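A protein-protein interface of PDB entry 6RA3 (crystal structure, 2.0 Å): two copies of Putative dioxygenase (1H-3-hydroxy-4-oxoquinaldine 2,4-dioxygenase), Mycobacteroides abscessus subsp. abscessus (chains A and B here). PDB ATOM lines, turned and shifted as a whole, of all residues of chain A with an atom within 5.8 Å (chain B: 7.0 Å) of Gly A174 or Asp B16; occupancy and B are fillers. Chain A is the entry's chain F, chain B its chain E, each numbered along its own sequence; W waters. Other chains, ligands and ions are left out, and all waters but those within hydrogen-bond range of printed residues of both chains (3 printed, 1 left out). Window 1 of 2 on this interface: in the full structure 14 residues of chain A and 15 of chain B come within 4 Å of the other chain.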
ATOM      1  N   ARG A  63      -3.111 -34.255   8.133  1.00  0.00           N
ATOM      2  CA  ARG A  63      -4.562 -34.297   8.265  1.00  0.00           C
ATOM      3  C   ARG A  63      -5.225 -34.610   6.944  1.00  0.00           C
ATOM      4  O   ARG A  63      -6.423 -34.348   6.768  1.00  0.00           O
ATOM      5  CB  ARG A  63      -5.099 -32.994   8.865  1.00  0.00           C
ATOM      6  CG  ARG A  63      -4.678 -32.793  10.321  1.00  0.00           C
ATOM      7  CD  ARG A  63      -5.230 -33.917  11.299  1.00  0.00           C
ATOM      8  NE  ARG A  63      -4.726 -33.624  12.624  1.00  0.00           N
ATOM      9  CZ  ARG A  63      -5.281 -32.776  13.477  1.00  0.00           C
ATOM     10  NH1 ARG A  63      -6.395 -32.163  13.159  1.00  0.00           N
ATOM     11  NH2 ARG A  63      -4.729 -32.561  14.673  1.00  0.00           N
ATOM     12  N   TYR A 170      -9.140 -25.352  21.992  1.00  0.00           N
ATOM     13  CA  TYR A 170      -8.014 -25.055  21.118  1.00  0.00           C
ATOM     14  C   TYR A 170      -7.246 -26.273  20.625  1.00  0.00           C
ATOM     15  O   TYR A 170      -6.398 -26.117  19.741  1.00  0.00           O
ATOM     16  CB  TYR A 170      -7.032 -24.108  21.832  1.00  0.00           C
ATOM     17  CG  TYR A 170      -7.709 -22.880  22.407  1.00  0.00           C
ATOM     18  CD1 TYR A 170      -8.728 -22.236  21.700  1.00  0.00           C
ATOM     19  CD2 TYR A 170      -7.371 -22.398  23.673  1.00  0.00           C
ATOM     20  CE1 TYR A 170      -9.392 -21.135  22.234  1.00  0.00           C
ATOM     21  CE2 TYR A 170      -8.015 -21.266  24.204  1.00  0.00           C
ATOM     22  CZ  TYR A 170      -9.024 -20.650  23.479  1.00  0.00           C
ATOM     23  OH  TYR A 170      -9.683 -19.557  23.989  1.00  0.00           O
ATOM     24  N   ASP A 171      -7.483 -27.468  21.168  1.00  0.00           N
ATOM     25  CA  ASP A 171      -6.698 -28.645  20.803  1.00  0.00           C
ATOM     26  C   ASP A 171      -7.505 -29.694  20.035  1.00  0.00           C
ATOM     27  O   ASP A 171      -7.050 -30.840  19.904  1.00  0.00           O
ATOM     28  CB  ASP A 171      -6.069 -29.278  22.046  1.00  0.00           C
ATOM     29  CG  ASP A 171      -5.096 -28.346  22.732  1.00  0.00           C
ATOM     30  OD1 ASP A 171      -4.752 -27.323  22.117  1.00  0.00           O
ATOM     31  OD2 ASP A 171      -4.701 -28.616  23.880  1.00  0.00           O
ATOM     32  N   SER A 172      -8.671 -29.340  19.495  1.00  0.00           N
ATOM     33  CA  SER A 172      -9.449 -30.311  18.719  1.00  0.00           C
ATOM     34  C   SER A 172      -9.753 -29.828  17.296  1.00  0.00           C
ATOM     35  O   SER A 172     -10.685 -30.322  16.662  1.00  0.00           O
ATOM     36  CB  SER A 172     -10.734 -30.690  19.454  1.00  0.00           C
ATOM     37  OG  SER A 172     -11.551 -29.589  19.675  1.00  0.00           O
ATOM     38  N   GLY A 173      -8.927 -28.935  16.757  1.00  0.00           N
ATOM     39  CA  GLY A 173      -9.133 -28.407  15.434  1.00  0.00           C
ATOM     40  C   GLY A 173      -8.474 -29.259  14.366  1.00  0.00           C
ATOM     41  O   GLY A 173      -7.826 -30.264  14.627  1.00  0.00           O
ATOM     42  N   GLY A 174      -8.715 -28.876  13.128  1.00  0.00           N
ATOM     43  CA  GLY A 174      -8.045 -29.511  12.014  1.00  0.00           C
ATOM     44  C   GLY A 174      -8.723 -30.743  11.470  1.00  0.00           C
ATOM     45  O   GLY A 174      -8.165 -31.376  10.554  1.00  0.00           O
ATOM     46  N   HIS A 175      -9.926 -31.064  11.951  1.00  0.00           N
ATOM     47  CA  HIS A 175     -10.729 -32.169  11.448  1.00  0.00           C
ATOM     48  C   HIS A 175     -11.992 -31.650  10.784  1.00  0.00           C
ATOM     49  O   HIS A 175     -12.540 -30.614  11.160  1.00  0.00           O
ATOM     50  CB  HIS A 175     -11.084 -33.155  12.567  1.00  0.00           C
ATOM     51  CG  HIS A 175      -9.893 -33.897  13.069  1.00  0.00           C
ATOM     52  ND1 HIS A 175      -9.152 -34.742  12.264  1.00  0.00           N
ATOM     53  CD2 HIS A 175      -9.253 -33.850  14.258  1.00  0.00           C
ATOM     54  CE1 HIS A 175      -8.144 -35.214  12.959  1.00  0.00           C
ATOM     55  NE2 HIS A 175      -8.190 -34.699  14.170  1.00  0.00           N
ATOM     56  N   GLY A 176     -12.425 -32.376   9.771  1.00  0.00           N
ATOM     57  CA  GLY A 176     -13.629 -32.025   9.052  1.00  0.00           C
ATOM     58  C   GLY A 176     -14.740 -33.045   9.226  1.00  0.00           C
ATOM     59  O   GLY A 176     -14.765 -33.846  10.191  1.00  0.00           O
ATOM     60  N   MET B   1       1.959 -29.321  16.977  1.00  0.00           N
ATOM     61  CA  MET B   1       1.040 -28.192  16.894  1.00  0.00           C
ATOM     62  C   MET B   1       0.552 -27.978  15.446  1.00  0.00           C
ATOM     63  O   MET B   1      -0.655 -27.814  15.180  1.00  0.00           O
ATOM     64  CB  MET B   1       1.734 -26.917  17.447  1.00  0.00           C
ATOM     65  N   THR B   3      -0.404 -28.626  11.566  1.00  0.00           N
ATOM     66  CA  THR B   3      -0.992 -29.661  10.738  1.00  0.00           C
ATOM     67  C   THR B   3      -0.840 -29.303   9.261  1.00  0.00           C
ATOM     68  O   THR B   3      -0.520 -28.158   8.893  1.00  0.00           O
ATOM     69  CB  THR B   3      -2.471 -29.885  11.157  1.00  0.00           C
ATOM     70  OG1 THR B   3      -3.173 -28.647  11.257  1.00  0.00           O
ATOM     71  CG2 THR B   3      -2.550 -30.514  12.551  1.00  0.00           C
ATOM     72  N   THR B   4      -0.991 -30.328   8.405  1.00  0.00           N
ATOM     73  CA  THR B   4      -0.876 -30.183   6.961  1.00  0.00           C
ATOM     74  C   THR B   4      -2.015 -30.898   6.260  1.00  0.00           C
ATOM     75  O   THR B   4      -2.480 -31.935   6.708  1.00  0.00           O
ATOM     76  CB  THR B   4       0.440 -30.767   6.410  1.00  0.00           C
ATOM     77  OG1 THR B   4       0.599 -32.134   6.818  1.00  0.00           O
ATOM     78  CG2 THR B   4       1.644 -29.958   6.887  1.00  0.00           C
ATOM     79  N   LYS B   5      -2.429 -30.366   5.133  1.00  0.00           N
ATOM     80  CA  LYS B   5      -3.314 -31.087   4.233  1.00  0.00           C
ATOM     81  C   LYS B   5      -2.815 -30.858   2.827  1.00  0.00           C
ATOM     82  O   LYS B   5      -2.240 -29.807   2.528  1.00  0.00           O
ATOM     83  CB  LYS B   5      -4.790 -30.624   4.301  1.00  0.00           C
ATOM     84  CG  LYS B   5      -5.617 -31.031   5.507  1.00  0.00           C
ATOM     85  CD  LYS B   5      -7.006 -30.540   5.268  1.00  0.00           C
ATOM     86  CE  LYS B   5      -7.941 -31.171   6.199  1.00  0.00           C
ATOM     87  NZ  LYS B   5      -8.306 -32.514   5.669  1.00  0.00           N
ATOM     88  N   PHE B  14      -1.036 -25.473   8.346  1.00  0.00           N
ATOM     89  CA  PHE B  14      -2.030 -24.592   8.949  1.00  0.00           C
ATOM     90  C   PHE B  14      -2.173 -24.997  10.405  1.00  0.00           C
ATOM     91  O   PHE B  14      -1.704 -26.060  10.813  1.00  0.00           O
ATOM     92  CB  PHE B  14      -3.352 -24.702   8.159  1.00  0.00           C
ATOM     93  CG  PHE B  14      -4.120 -26.016   8.417  1.00  0.00           C
ATOM     94  CD1 PHE B  14      -3.844 -27.157   7.681  1.00  0.00           C
ATOM     95  CD2 PHE B  14      -5.075 -26.083   9.417  1.00  0.00           C
ATOM     96  CE1 PHE B  14      -4.515 -28.357   7.923  1.00  0.00           C
ATOM     97  CE2 PHE B  14      -5.764 -27.256   9.681  1.00  0.00           C
ATOM     98  CZ  PHE B  14      -5.479 -28.410   8.919  1.00  0.00           C
ATOM     99  N   ASP B  15      -2.863 -24.178  11.192  1.00  0.00           N
ATOM    100  CA  ASP B  15      -3.385 -24.721  12.426  1.00  0.00           C
ATOM    101  C   ASP B  15      -4.737 -24.075  12.718  1.00  0.00           C
ATOM    102  O   ASP B  15      -5.080 -23.010  12.199  1.00  0.00           O
ATOM    103  CB  ASP B  15      -2.371 -24.662  13.591  1.00  0.00           C
ATOM    104  CG  ASP B  15      -2.152 -23.283  14.166  1.00  0.00           C
ATOM    105  OD1 ASP B  15      -2.597 -22.280  13.585  1.00  0.00           O
ATOM    106  OD2 ASP B  15      -1.513 -23.216  15.252  1.00  0.00           O
ATOM    107  N   ASP B  16      -5.541 -24.797  13.492  1.00  0.00           N
ATOM    108  CA  ASP B  16      -6.958 -24.495  13.637  1.00  0.00           C
ATOM    109  C   ASP B  16      -7.273 -24.591  15.115  1.00  0.00           C
ATOM    110  O   ASP B  16      -7.089 -25.652  15.712  1.00  0.00           O
ATOM    111  CB  ASP B  16      -7.780 -25.466  12.789  1.00  0.00           C
ATOM    112  CG  ASP B  16      -9.268 -25.386  13.062  1.00  0.00           C
ATOM    113  OD1 ASP B  16      -9.754 -24.353  13.591  1.00  0.00           O
ATOM    114  OD2 ASP B  16      -9.971 -26.363  12.710  1.00  0.00           O
ATOM    115  N   GLN B  17      -7.711 -23.481  15.709  1.00  0.00           N
ATOM    116  CA  GLN B  17      -7.899 -23.378  17.147  1.00  0.00           C
ATOM    117  C   GLN B  17      -9.145 -22.562  17.416  1.00  0.00           C
ATOM    118  O   GLN B  17      -9.387 -21.553  16.743  1.00  0.00           O
ATOM    119  CB  GLN B  17      -6.710 -22.692  17.839  1.00  0.00           C
ATOM    120  CG  GLN B  17      -5.397 -23.444  17.659  1.00  0.00           C
ATOM    121  CD  GLN B  17      -4.235 -22.880  18.462  1.00  0.00           C
ATOM    122  OE1 GLN B  17      -4.353 -22.583  19.643  1.00  0.00           O
ATOM    123  NE2 GLN B  17      -3.089 -22.761  17.811  1.00  0.00           N
ATOM    124  N   GLY B  18      -9.893 -22.942  18.442  1.00  0.00           N
ATOM    125  CA  GLY B  18     -11.044 -22.142  18.807  1.00  0.00           C
ATOM    126  C   GLY B  18     -12.346 -22.765  18.350  1.00  0.00           C
ATOM    127  O   GLY B  18     -12.408 -23.575  17.426  1.00  0.00           O
ATOM    128  N   HIS B  19     -13.393 -22.377  19.046  1.00  0.00           N
ATOM    129  CA  HIS B  19     -14.727 -22.895  18.821  1.00  0.00           C
ATOM    130  C   HIS B  19     -15.628 -21.810  19.377  1.00  0.00           C
ATOM    131  O   HIS B  19     -15.686 -21.608  20.595  1.00  0.00           O
ATOM    132  CB  HIS B  19     -14.942 -24.228  19.518  1.00  0.00           C
ATOM    133  CG  HIS B  19     -16.248 -24.857  19.186  1.00  0.00           C
ATOM    134  ND1 HIS B  19     -17.330 -24.816  20.039  1.00  0.00           N
ATOM    135  CD2 HIS B  19     -16.664 -25.506  18.075  1.00  0.00           C
ATOM    136  CE1 HIS B  19     -18.354 -25.433  19.476  1.00  0.00           C
ATOM    137  NE2 HIS B  19     -17.978 -25.858  18.281  1.00  0.00           N
ATOM    138  N   VAL B  24     -14.934 -17.145  10.998  1.00  0.00           N
ATOM    139  CA  VAL B  24     -13.625 -17.649  11.366  1.00  0.00           C
ATOM    140  C   VAL B  24     -12.551 -16.637  10.973  1.00  0.00           C
ATOM    141  O   VAL B  24     -12.553 -16.121   9.850  1.00  0.00           O
ATOM    142  CB  VAL B  24     -13.404 -19.010  10.679  1.00  0.00           C
ATOM    143  CG1 VAL B  24     -11.989 -19.505  10.867  1.00  0.00           C
ATOM    144  CG2 VAL B  24     -14.471 -20.011  11.190  1.00  0.00           C
ATOM    145  N   ARG B  50     -13.101 -18.887  16.350  1.00  0.00           N
ATOM    146  CA  ARG B  50     -12.270 -19.917  15.737  1.00  0.00           C
ATOM    147  C   ARG B  50     -11.288 -19.261  14.785  1.00  0.00           C
ATOM    148  O   ARG B  50     -11.667 -18.405  13.982  1.00  0.00           O
ATOM    149  CB  ARG B  50     -13.133 -20.942  14.980  1.00  0.00           C
ATOM    150  CG  ARG B  50     -12.328 -21.993  14.234  1.00  0.00           C
ATOM    151  CD  ARG B  50     -13.280 -22.947  13.531  1.00  0.00           C
ATOM    152  NE  ARG B  50     -12.576 -24.052  12.873  1.00  0.00           N
ATOM    153  CZ  ARG B  50     -13.162 -24.877  12.012  1.00  0.00           C
ATOM    154  NH1 ARG B  50     -14.457 -24.764  11.758  1.00  0.00           N
ATOM    155  NH2 ARG B  50     -12.474 -25.832  11.438  1.00  0.00           N
ATOM    156  N   THR B  51     -10.025 -19.655  14.882  1.00  0.00           N
ATOM    157  CA  THR B  51      -8.943 -19.040  14.117  1.00  0.00           C
ATOM    158  C   THR B  51      -8.154 -20.104  13.369  1.00  0.00           C
ATOM    159  O   THR B  51      -7.616 -21.032  13.980  1.00  0.00           O
ATOM    160  CB  THR B  51      -8.039 -18.237  15.053  1.00  0.00           C
ATOM    161  OG1 THR B  51      -8.784 -17.149  15.572  1.00  0.00           O
ATOM    162  CG2 THR B  51      -6.848 -17.692  14.321  1.00  0.00           C
ATOM    163  N   VAL B  52      -8.089 -19.964  12.049  1.00  0.00           N
ATOM    164  CA  VAL B  52      -7.277 -20.835  11.206  1.00  0.00           C
ATOM    165  C   VAL B  52      -6.106 -20.023  10.655  1.00  0.00           C
ATOM    166  O   VAL B  52      -6.288 -19.074   9.871  1.00  0.00           O
ATOM    167  CB  VAL B  52      -8.136 -21.470  10.095  1.00  0.00           C
ATOM    168  CG1 VAL B  52      -7.339 -22.409   9.200  1.00  0.00           C
ATOM    169  CG2 VAL B  52      -9.272 -22.220  10.712  1.00  0.00           C
ATOM    170  N   ARG B  53      -4.898 -20.367  11.080  1.00  0.00           N
ATOM    171  CA  ARG B  53      -3.679 -19.778  10.539  1.00  0.00           C
ATOM    172  C   ARG B  53      -3.170 -20.614   9.381  1.00  0.00           C
ATOM    173  O   ARG B  53      -3.014 -21.836   9.515  1.00  0.00           O
ATOM    174  CB  ARG B  53      -2.608 -19.683  11.605  1.00  0.00           C
ATOM    175  CG  ARG B  53      -3.052 -18.931  12.835  1.00  0.00           C
ATOM    176  CD  ARG B  53      -1.878 -18.614  13.729  1.00  0.00           C
ATOM    177  NE  ARG B  53      -1.329 -19.824  14.326  1.00  0.00           N
ATOM    178  CZ  ARG B  53      -0.208 -19.896  15.033  1.00  0.00           C
ATOM    179  NH1 ARG B  53       0.570 -18.814  15.235  1.00  0.00           N
ATOM    180  NH2 ARG B  53       0.138 -21.072  15.541  1.00  0.00           N
ATOM    181  N   LEU B  85     -12.051 -28.042   5.369  1.00  0.00           N
ATOM    182  CA  LEU B  85     -12.498 -27.970   6.752  1.00  0.00           C
ATOM    183  C   LEU B  85     -13.972 -27.591   6.890  1.00  0.00           C
ATOM    184  O   LEU B  85     -14.510 -27.618   8.013  1.00  0.00           O
ATOM    185  CB  LEU B  85     -11.643 -26.957   7.490  1.00  0.00           C
ATOM    186  CG  LEU B  85     -10.171 -27.313   7.608  1.00  0.00           C
ATOM    187  CD1 LEU B  85      -9.382 -26.118   8.088  1.00  0.00           C
ATOM    188  CD2 LEU B  85     -10.081 -28.508   8.567  1.00  0.00           C
ATOM    189  N   VAL B  87     -15.217 -24.605   6.613  1.00  0.00           N
ATOM    190  CA  VAL B  87     -15.382 -23.258   7.148  1.00  0.00           C
ATOM    191  C   VAL B  87     -16.378 -22.512   6.267  1.00  0.00           C
ATOM    192  O   VAL B  87     -16.283 -22.552   5.045  1.00  0.00           O
ATOM    193  CB  VAL B  87     -14.013 -22.553   7.194  1.00  0.00           C
ATOM    194  CG1 VAL B  87     -14.211 -21.067   7.482  1.00  0.00           C
ATOM    195  CG2 VAL B  87     -13.132 -23.224   8.219  1.00  0.00           C
HETATM  196  O   HOH W   1      -9.014 -32.718   8.413  1.00  0.00           O
HETATM  197  O   HOH W   2      -6.396 -27.526  17.514  1.00  0.00           O
HETATM  198  O   HOH W   3     -13.772 -28.259  10.555  1.00  0.00           O
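The backbone NH (N) of Gly A174 sits at hydrogen-bond distance from the side-chain carboxylate (OD2) of Asp B16, 2.8 Å away. The backbone NH of Arg A63 is in hydrogen-bond range of the backbone carbonyl oxygen of Thr B4, 2.8 Å away. NZ of Lys B5 sits at hydrogen-bond distance from O of Arg A63.
NH1 of Arg A63 lies within hydrogen-bond range of NE2 of His A175. N of Phe B14 sits at hydrogen-bond distance from O of Thr B3 (2.8 Å). The guanidinium group of Arg A63 sits close to the backbone carbonyl oxygen of Gly A174. NH1 of Arg A63 sits at hydrogen-bond distance from O of Gly A173, at 2.8 Å. The side-chain amide nitrogen (NE2) of Gln B17 lies within hydrogen-bond range of the side-chain carboxylate (OD2) of Asp B15. The backbone carbonyl oxygen of Gln B17 sits at hydrogen-bond distance from the backbone NH of Thr B51.
Among the printed residues, pairs that only touch across the chains: Gly A173 with Asp B16, Tyr A170 with Gly B18, Tyr A170 with Gln B17, Arg A63 with Thr B3, Gly A174 with Leu B85 and Gly A174 with Phe B14.
Gly A174 touches just these residues of chain B: Phe B14, Asp B16 and Leu B85. Of chain A, only Gly A173 (3.4 Å) and Gly A174 (2.8 Å) come within 4 Å of Asp B16. Of the printed residues of chain A, Gln B17 touches Tyr A170. Of the printed residues of chain B, Tyr A170 touches Gln B17 (3.5 Å) and Gly B18 (3.5 Å). Printed residues of chain A within 4 Å of Gly B18: Tyr A170 (3.5 Å). Of the printed residues of chain A, Leu B85 touches Gly A174 (3.9 Å). The nearest residue of chain B that does not touch Gly A174 is Lys B5 (4.4 Å). The nearest residue of chain A that does not touch Asp B16 is Tyr A170 (4.1 Å). The nearest printed residue of chain A that does not touch Thr B4 is Gly A174 (6.9 Å).
Printed residues of chain A that touch a printed residue of chain B: Arg A63, Tyr A170, Gly A173 and Gly A174. Along chain A the printed residues that touch a printed residue of chain B span positions 63 to 174. Of the 17 printed residues of chain B, 8 touch a printed residue of chain A. Printed residues of chain B that touch a printed residue of chain A: Thr B3, Thr B4, Lys B5, Phe B14, Asp B16, Gln B17, Gly B18 and Leu B85. Among the printed residues, 9 pairs touch across the chains. Among the printed residues, no Asp or Glu carboxylate lies within 4 Å of a Lys or Arg side-chain nitrogen of the other chain.
No position is printed for both chains. Of the 9 pairs that touch across the chains among the printed residues, none has its exchanged pair printed and touching as well.
Water W2 lies within hydrogen-bond range of O of Tyr A170 (2.6 Å), O of Asp B16 (2.7 Å) and N of Gly A173 (3.0 Å). Water W1 lies within hydrogen-bond range of the backbone carbonyl oxygen (O) of Gly A174 (2.7 Å), the side-chain amino group (NZ) of Lys B5 (2.8 Å) and the backbone carbonyl oxygen (O) of Arg A63 (3.5 Å). Water W3 lies within hydrogen-bond range of the backbone carbonyl oxygen (O) of Leu B85, the backbone carbonyl oxygen (O) of His A175 and the guanidinium group (NH2) of Arg B50.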
